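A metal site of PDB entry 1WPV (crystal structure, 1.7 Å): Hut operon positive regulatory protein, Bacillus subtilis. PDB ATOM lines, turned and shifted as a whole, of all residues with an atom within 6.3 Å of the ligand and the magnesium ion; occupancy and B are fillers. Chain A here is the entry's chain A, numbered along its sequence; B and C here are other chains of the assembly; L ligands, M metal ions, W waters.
A nitrogen (N1) of the ligand is in hydrogen-bond range of the side-chain hydroxyl (OH) of Tyr 68, 2.7 Å away.
The guanidinium group (NH2) of Arg 87 of chain B lies within salt-bridge range of an oxygen (O2) of the ligand, at 2.9 Å.
An oxygen (O2) of the ligand is in salt-bridge range of the guanidinium group of Arg 97 of chain B, at 2.9 Å.
A nitrogen (N2) of the ligand sits close to the backbone NH (N) of Ala 130 of chain B (3.4 Å).
N of Ile 128 of chain B is in hydrogen-bond range of O of His 137 of chain B, 2.9 Å away.
OE1 of Glu 80 of chain C is in salt-bridge range of NH1 of Arg 87 of chain B (3.1 Å).
NH2 of Arg 97 of chain B sits at hydrogen-bond distance from O of Thr 86 of chain B (3.1 Å).
The side-chain hydroxyl of Tyr 75 lies within hydrogen-bond range of the backbone carbonyl oxygen of Leu 95 of chain B (2.7 Å).
N of Ala 130 of chain B sits at hydrogen-bond distance from O of Leu 135 of chain B (2.9 Å).
The backbone carbonyl oxygen (O) of Gly 129 of chain B is in hydrogen-bond range of the backbone NH (N) of Thr 98 of chain B (2.8 Å).
Merely in contact with the ligand: Tyr 75 (3.4 Å), Gly 129 of chain B (3.5 Å) and Ile 128 of chain B (3.5 Å).
Hydrophobic or aromatic side chains that line the ligand: Tyr 68, Tyr 75, His 76, Ile 128 of chain B, Ala 130 of chain B and His 137 of chain B.
Of the 23 residues printed, 9 come within 4 Å of the ligand.
The nearest printed residue that does not touch the ligand is Leu 96 of chain B (4.02 Å).
Of the 23 residues printed, 3 come within 4 Å of the magnesium ion.
The magnesium ion is bound by an oxygen (O1) of the ligand (2.2 Å), water W1 (2.2 Å), a ring nitrogen (NE2) of His 72 (2.2 Å), a ring nitrogen (NE2) of His 76 (2.2 Å) and a ring nitrogen (NE2) of His 137 of chain B (2.3 Å).
Water W1 lies within hydrogen-bond range of the backbone carbonyl oxygen (O) of Ile 144 of chain C and the side-chain carboxylate (OE1) of Glu 80 of chain C.
Water W2 lies within hydrogen-bond range of O of Leu 96 of chain B and N2 of the ligand.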
ATOM      1  N   TYR A  68      22.401  11.855  -0.614  1.00  0.00           N
ATOM      2  CA  TYR A  68      22.400  12.524   0.682  1.00  0.00           C
ATOM      3  C   TYR A  68      21.263  12.030   1.567  1.00  0.00           C
ATOM      4  O   TYR A  68      21.447  11.863   2.767  1.00  0.00           O
ATOM      5  CB  TYR A  68      22.280  14.035   0.464  1.00  0.00           C
ATOM      6  CG  TYR A  68      22.317  14.860   1.731  1.00  0.00           C
ATOM      7  CD1 TYR A  68      23.195  14.555   2.773  1.00  0.00           C
ATOM      8  CD2 TYR A  68      21.513  15.998   1.857  1.00  0.00           C
ATOM      9  CE1 TYR A  68      23.280  15.362   3.891  1.00  0.00           C
ATOM     10  CE2 TYR A  68      21.593  16.812   2.980  1.00  0.00           C
ATOM     11  CZ  TYR A  68      22.473  16.490   3.990  1.00  0.00           C
ATOM     12  OH  TYR A  68      22.577  17.304   5.095  1.00  0.00           O
ATOM     13  N   SER A  71      21.937   9.480   4.261  1.00  0.00           N
ATOM     14  CA  SER A  71      22.958  10.029   5.147  1.00  0.00           C
ATOM     15  C   SER A  71      22.303  11.083   6.039  1.00  0.00           C
ATOM     16  O   SER A  71      22.617  11.190   7.227  1.00  0.00           O
ATOM     17  CB  SER A  71      24.086  10.664   4.329  1.00  0.00           C
ATOM     18  OG  SER A  71      24.847   9.676   3.644  1.00  0.00           O
ATOM     19  N   HIS A  72      21.384  11.854   5.464  1.00  0.00           N
ATOM     20  CA  HIS A  72      20.700  12.878   6.231  1.00  0.00           C
ATOM     21  C   HIS A  72      19.841  12.225   7.313  1.00  0.00           C
ATOM     22  O   HIS A  72      19.854  12.661   8.458  1.00  0.00           O
ATOM     23  CB  HIS A  72      19.827  13.739   5.310  1.00  0.00           C
ATOM     24  CG  HIS A  72      19.255  14.937   5.993  1.00  0.00           C
ATOM     25  ND1 HIS A  72      17.961  14.974   6.481  1.00  0.00           N
ATOM     26  CD2 HIS A  72      19.809  16.129   6.303  1.00  0.00           C
ATOM     27  CE1 HIS A  72      17.748  16.136   7.060  1.00  0.00           C
ATOM     28  NE2 HIS A  72      18.857  16.856   6.962  1.00  0.00           N
ATOM     29  N   TYR A  75      22.173  10.964  10.014  1.00  0.00           N
ATOM     30  CA  TYR A  75      22.800  12.024  10.803  1.00  0.00           C
ATOM     31  C   TYR A  75      21.863  12.510  11.886  1.00  0.00           C
ATOM     32  O   TYR A  75      22.239  12.631  13.055  1.00  0.00           O
ATOM     33  CB  TYR A  75      23.211  13.200   9.898  1.00  0.00           C
ATOM     34  CG  TYR A  75      23.911  14.318  10.655  1.00  0.00           C
ATOM     35  CD1 TYR A  75      25.283  14.262  10.891  1.00  0.00           C
ATOM     36  CD2 TYR A  75      23.205  15.416  11.154  1.00  0.00           C
ATOM     37  CE1 TYR A  75      25.936  15.269  11.623  1.00  0.00           C
ATOM     38  CE2 TYR A  75      23.847  16.423  11.876  1.00  0.00           C
ATOM     39  CZ  TYR A  75      25.214  16.337  12.109  1.00  0.00           C
ATOM     40  OH  TYR A  75      25.860  17.337  12.827  1.00  0.00           O
ATOM     41  N   HIS A  76      20.629  12.803  11.501  1.00  0.00           N
ATOM     42  CA  HIS A  76      19.692  13.284  12.489  1.00  0.00           C
ATOM     43  C   HIS A  76      19.307  12.243  13.506  1.00  0.00           C
ATOM     44  O   HIS A  76      19.081  12.569  14.660  1.00  0.00           O
ATOM     45  CB  HIS A  76      18.487  13.884  11.808  1.00  0.00           C
ATOM     46  CG  HIS A  76      18.758  15.256  11.285  1.00  0.00           C
ATOM     47  ND1 HIS A  76      18.869  16.351  12.111  1.00  0.00           N
ATOM     48  CD2 HIS A  76      19.056  15.678  10.039  1.00  0.00           C
ATOM     49  CE1 HIS A  76      19.223  17.400  11.394  1.00  0.00           C
ATOM     50  NE2 HIS A  76      19.347  17.025  10.133  1.00  0.00           N
ATOM     51  N   VAL B  85      20.775  28.731  12.138  1.00  0.00           N
ATOM     52  CA  VAL B  85      21.666  27.915  11.329  1.00  0.00           C
ATOM     53  C   VAL B  85      21.970  26.579  11.991  1.00  0.00           C
ATOM     54  O   VAL B  85      21.932  25.531  11.347  1.00  0.00           O
ATOM     55  CB  VAL B  85      23.009  28.658  11.062  1.00  0.00           C
ATOM     56  CG1 VAL B  85      24.060  27.696  10.496  1.00  0.00           C
ATOM     57  CG2 VAL B  85      22.777  29.803  10.084  1.00  0.00           C
ATOM     58  N   THR B  86      22.262  26.607  13.292  1.00  0.00           N
ATOM     59  CA  THR B  86      22.616  25.376  14.010  1.00  0.00           C
ATOM     60  C   THR B  86      21.449  24.586  14.594  1.00  0.00           C
ATOM     61  O   THR B  86      21.577  23.387  14.849  1.00  0.00           O
ATOM     62  CB  THR B  86      23.601  25.698  15.131  1.00  0.00           C
ATOM     63  OG1 THR B  86      23.022  26.669  15.995  1.00  0.00           O
ATOM     64  CG2 THR B  86      24.899  26.232  14.542  1.00  0.00           C
ATOM     65  N   ARG B  87      20.318  25.245  14.819  1.00  0.00           N
ATOM     66  CA  ARG B  87      19.117  24.562  15.317  1.00  0.00           C
ATOM     67  C   ARG B  87      19.291  23.618  16.509  1.00  0.00           C
ATOM     68  O   ARG B  87      18.977  22.426  16.409  1.00  0.00           O
ATOM     69  CB  ARG B  87      18.450  23.796  14.162  1.00  0.00           C
ATOM     70  CG  ARG B  87      17.768  24.687  13.120  1.00  0.00           C
ATOM     71  CD  ARG B  87      17.917  24.115  11.725  1.00  0.00           C
ATOM     72  NE  ARG B  87      19.329  24.043  11.341  1.00  0.00           N
ATOM     73  CZ  ARG B  87      19.935  22.941  10.933  1.00  0.00           C
ATOM     74  NH1 ARG B  87      19.266  21.795  10.826  1.00  0.00           N
ATOM     75  NH2 ARG B  87      21.244  22.965  10.672  1.00  0.00           N
ATOM     76  N   LEU B  95      30.492  18.448  15.442  1.00  0.00           N
ATOM     77  CA  LEU B  95      29.358  17.572  15.161  1.00  0.00           C
ATOM     78  C   LEU B  95      29.433  17.090  13.727  1.00  0.00           C
ATOM     79  O   LEU B  95      28.436  16.712  13.136  1.00  0.00           O
ATOM     80  CB  LEU B  95      28.028  18.287  15.394  1.00  0.00           C
ATOM     81  CG  LEU B  95      27.674  18.668  16.828  1.00  0.00           C
ATOM     82  CD1 LEU B  95      26.218  19.116  16.867  1.00  0.00           C
ATOM     83  CD2 LEU B  95      27.883  17.470  17.760  1.00  0.00           C
ATOM     84  N   LEU B  96      30.636  17.117  13.179  1.00  0.00           N
ATOM     85  CA  LEU B  96      30.895  16.669  11.813  1.00  0.00           C
ATOM     86  C   LEU B  96      30.093  17.395  10.734  1.00  0.00           C
ATOM     87  O   LEU B  96      29.659  16.778   9.766  1.00  0.00           O
ATOM     88  CB  LEU B  96      30.666  15.161  11.710  1.00  0.00           C
ATOM     89  CG  LEU B  96      31.482  14.451  10.616  1.00  0.00           C
ATOM     90  CD1 LEU B  96      32.962  14.701  10.852  1.00  0.00           C
ATOM     91  CD2 LEU B  96      31.203  12.952  10.634  1.00  0.00           C
ATOM     92  N   ARG B  97      29.904  18.695  10.895  1.00  0.00           N
ATOM     93  CA  ARG B  97      29.206  19.455   9.867  1.00  0.00           C
ATOM     94  C   ARG B  97      29.943  20.758   9.591  1.00  0.00           C
ATOM     95  O   ARG B  97      30.690  21.265  10.415  1.00  0.00           O
ATOM     96  CB  ARG B  97      27.727  19.697  10.242  1.00  0.00           C
ATOM     97  CG  ARG B  97      27.475  20.476  11.517  1.00  0.00           C
ATOM     98  CD  ARG B  97      25.969  20.625  11.779  1.00  0.00           C
ATOM     99  NE  ARG B  97      25.724  21.317  13.029  1.00  0.00           N
ATOM    100  CZ  ARG B  97      24.525  21.561  13.547  1.00  0.00           C
ATOM    101  NH1 ARG B  97      23.433  21.172  12.902  1.00  0.00           N
ATOM    102  NH2 ARG B  97      24.417  22.195  14.711  1.00  0.00           N
ATOM    103  N   THR B  98      29.712  21.309   8.411  1.00  0.00           N
ATOM    104  CA  THR B  98      30.376  22.535   8.017  1.00  0.00           C
ATOM    105  C   THR B  98      29.382  23.446   7.327  1.00  0.00           C
ATOM    106  O   THR B  98      28.379  22.973   6.789  1.00  0.00           O
ATOM    107  CB  THR B  98      31.534  22.192   7.039  1.00  0.00           C
ATOM    108  OG1 THR B  98      32.261  23.382   6.716  1.00  0.00           O
ATOM    109  CG2 THR B  98      30.986  21.554   5.774  1.00  0.00           C
ATOM    110  N   ILE B 128      24.604  23.847   5.067  1.00  0.00           N
ATOM    111  CA  ILE B 128      25.166  23.194   6.230  1.00  0.00           C
ATOM    112  C   ILE B 128      25.117  21.724   5.827  1.00  0.00           C
ATOM    113  O   ILE B 128      24.144  21.267   5.233  1.00  0.00           O
ATOM    114  CB  ILE B 128      24.333  23.461   7.508  1.00  0.00           C
ATOM    115  CG1 ILE B 128      25.074  22.894   8.721  1.00  0.00           C
ATOM    116  CG2 ILE B 128      22.943  22.833   7.385  1.00  0.00           C
ATOM    117  CD1 ILE B 128      24.618  23.439  10.058  1.00  0.00           C
ATOM    118  N   GLY B 129      26.192  20.990   6.096  1.00  0.00           N
ATOM    119  CA  GLY B 129      26.214  19.593   5.714  1.00  0.00           C
ATOM    120  C   GLY B 129      27.493  18.891   6.114  1.00  0.00           C
ATOM    121  O   GLY B 129      28.285  19.408   6.887  1.00  0.00           O
ATOM    122  N   ALA B 130      27.677  17.692   5.580  1.00  0.00           N
ATOM    123  CA  ALA B 130      28.858  16.897   5.861  1.00  0.00           C
ATOM    124  C   ALA B 130      30.084  17.537   5.230  1.00  0.00           C
ATOM    125  O   ALA B 130      29.983  18.324   4.296  1.00  0.00           O
ATOM    126  CB  ALA B 130      28.668  15.487   5.314  1.00  0.00           C
ATOM    127  N   PRO B 131      31.277  17.194   5.749  1.00  0.00           N
ATOM    128  CA  PRO B 131      32.530  17.740   5.200  1.00  0.00           C
ATOM    129  C   PRO B 131      32.629  17.439   3.707  1.00  0.00           C
ATOM    130  O   PRO B 131      33.103  18.260   2.934  1.00  0.00           O
ATOM    131  CB  PRO B 131      33.586  17.019   6.014  1.00  0.00           C
ATOM    132  CG  PRO B 131      32.916  16.832   7.346  1.00  0.00           C
ATOM    133  CD  PRO B 131      31.531  16.387   6.960  1.00  0.00           C
ATOM    134  N   LEU B 135      26.704  16.515   0.119  1.00  0.00           N
ATOM    135  CA  LEU B 135      25.886  16.078   1.249  1.00  0.00           C
ATOM    136  C   LEU B 135      25.540  17.264   2.127  1.00  0.00           C
ATOM    137  O   LEU B 135      26.128  17.457   3.192  1.00  0.00           O
ATOM    138  CB  LEU B 135      26.630  15.020   2.071  1.00  0.00           C
ATOM    139  CG  LEU B 135      27.152  13.773   1.351  1.00  0.00           C
ATOM    140  CD1 LEU B 135      27.729  12.825   2.375  1.00  0.00           C
ATOM    141  CD2 LEU B 135      26.030  13.101   0.585  1.00  0.00           C
ATOM    142  N   GLU B 136      24.560  18.055   1.704  1.00  0.00           N
ATOM    143  CA  GLU B 136      24.200  19.219   2.480  1.00  0.00           C
ATOM    144  C   GLU B 136      22.846  19.777   2.056  1.00  0.00           C
ATOM    145  O   GLU B 136      22.312  19.394   1.016  1.00  0.00           O
ATOM    146  CB  GLU B 136      25.255  20.296   2.274  1.00  0.00           C
ATOM    147  CG  GLU B 136      25.140  20.939   0.873  1.00  0.00           C
ATOM    148  CD  GLU B 136      26.482  21.160   0.199  1.00  0.00           C
ATOM    149  OE1 GLU B 136      27.499  20.593   0.652  1.00  0.00           O
ATOM    150  OE2 GLU B 136      26.512  21.895  -0.816  1.00  0.00           O
ATOM    151  N   HIS B 137      22.298  20.666   2.869  1.00  0.00           N
ATOM    152  CA  HIS B 137      21.061  21.348   2.519  1.00  0.00           C
ATOM    153  C   HIS B 137      21.212  22.797   2.991  1.00  0.00           C
ATOM    154  O   HIS B 137      22.216  23.161   3.608  1.00  0.00           O
ATOM    155  CB  HIS B 137      19.821  20.659   3.127  1.00  0.00           C
ATOM    156  CG  HIS B 137      19.814  20.591   4.621  1.00  0.00           C
ATOM    157  ND1 HIS B 137      19.711  21.715   5.420  1.00  0.00           N
ATOM    158  CD2 HIS B 137      19.851  19.536   5.461  1.00  0.00           C
ATOM    159  CE1 HIS B 137      19.688  21.339   6.683  1.00  0.00           C
ATOM    160  NE2 HIS B 137      19.773  20.027   6.739  1.00  0.00           N
ATOM    161  N   GLU C  80      12.664  22.642  13.545  1.00  0.00           N
ATOM    162  CA  GLU C  80      13.895  23.301  13.132  1.00  0.00           C
ATOM    163  C   GLU C  80      13.636  24.766  12.806  1.00  0.00           C
ATOM    164  O   GLU C  80      14.428  25.632  13.175  1.00  0.00           O
ATOM    165  CB  GLU C  80      14.524  22.546  11.942  1.00  0.00           C
ATOM    166  CG  GLU C  80      15.061  21.171  12.343  1.00  0.00           C
ATOM    167  CD  GLU C  80      16.036  20.593  11.329  1.00  0.00           C
ATOM    168  OE1 GLU C  80      16.229  21.222  10.264  1.00  0.00           O
ATOM    169  N   TRP C 119      11.884  16.613  -0.520  1.00  0.00           N
ATOM    170  CA  TRP C 119      12.362  17.238   0.698  1.00  0.00           C
ATOM    171  C   TRP C 119      11.310  18.294   1.025  1.00  0.00           C
ATOM    172  O   TRP C 119      10.508  18.658   0.169  1.00  0.00           O
ATOM    173  CB  TRP C 119      13.729  17.891   0.504  1.00  0.00           C
ATOM    174  CG  TRP C 119      14.818  16.899   0.399  1.00  0.00           C
ATOM    175  CD1 TRP C 119      15.006  15.994  -0.615  1.00  0.00           C
ATOM    176  CD2 TRP C 119      15.863  16.661   1.346  1.00  0.00           C
ATOM    177  NE1 TRP C 119      16.103  15.206  -0.346  1.00  0.00           N
ATOM    178  CE2 TRP C 119      16.644  15.593   0.857  1.00  0.00           C
ATOM    179  CE3 TRP C 119      16.203  17.243   2.573  1.00  0.00           C
ATOM    180  CZ2 TRP C 119      17.754  15.092   1.543  1.00  0.00           C
ATOM    181  CZ3 TRP C 119      17.312  16.743   3.259  1.00  0.00           C
ATOM    182  CH2 TRP C 119      18.063  15.689   2.739  1.00  0.00           C
ATOM    183  N   ILE C 144      14.527  22.397   7.252  1.00  0.00           N
ATOM    184  CA  ILE C 144      14.538  21.582   6.038  1.00  0.00           C
ATOM    185  C   ILE C 144      14.674  20.101   6.407  1.00  0.00           C
ATOM    186  O   ILE C 144      15.473  19.739   7.276  1.00  0.00           O
ATOM    187  CB  ILE C 144      15.689  22.041   5.096  1.00  0.00           C
ATOM    188  CG1 ILE C 144      15.308  23.399   4.488  1.00  0.00           C
ATOM    189  CG2 ILE C 144      15.929  21.005   4.000  1.00  0.00           C
ATOM    190  CD1 ILE C 144      16.401  24.070   3.685  1.00  0.00           C
ATOM    191  N   ASN C 145      13.889  19.244   5.752  1.00  0.00           N
ATOM    192  CA  ASN C 145      13.924  17.821   6.061  1.00  0.00           C
ATOM    193  C   ASN C 145      13.604  16.995   4.826  1.00  0.00           C
ATOM    194  O   ASN C 145      12.989  17.490   3.881  1.00  0.00           O
ATOM    195  CB  ASN C 145      12.900  17.518   7.160  1.00  0.00           C
ATOM    196  CG  ASN C 145      13.256  16.286   7.981  1.00  0.00           C
ATOM    197  OD1 ASN C 145      14.301  15.687   7.808  1.00  0.00           O
ATOM    198  ND2 ASN C 145      12.360  15.911   8.907  1.00  0.00           N
HETATM  199  C1  LIG L   1      22.609  18.359   9.149  1.00  0.00           C
HETATM  200  C2  LIG L   1      21.938  19.629   9.674  1.00  0.00           C
HETATM  201  O1  LIG L   1      20.694  19.719   9.611  1.00  0.00           O
HETATM  202  C3  LIG L   1      23.935  18.707   8.455  1.00  0.00           C
HETATM  203  C4  LIG L   1      24.732  17.500   8.061  1.00  0.00           C
HETATM  204  N1  LIG L   1      24.373  16.695   6.998  1.00  0.00           N
HETATM  205  C5  LIG L   1      25.807  16.919   8.632  1.00  0.00           C
HETATM  206  C6  LIG L   1      25.192  15.656   6.944  1.00  0.00           C
HETATM  207  N2  LIG L   1      26.072  15.766   7.930  1.00  0.00           N
HETATM  208  O2  LIG L   1      22.673  20.515  10.159  1.00  0.00           O
HETATM  209 MG    MG M   1      19.549  18.380   8.366  1.00  0.00          MG
HETATM  210  O   HOH W   1      17.608  19.198   8.845  1.00  0.00           O
HETATM  211  O   HOH W   2      28.462  14.530   8.685  1.00  0.00           O
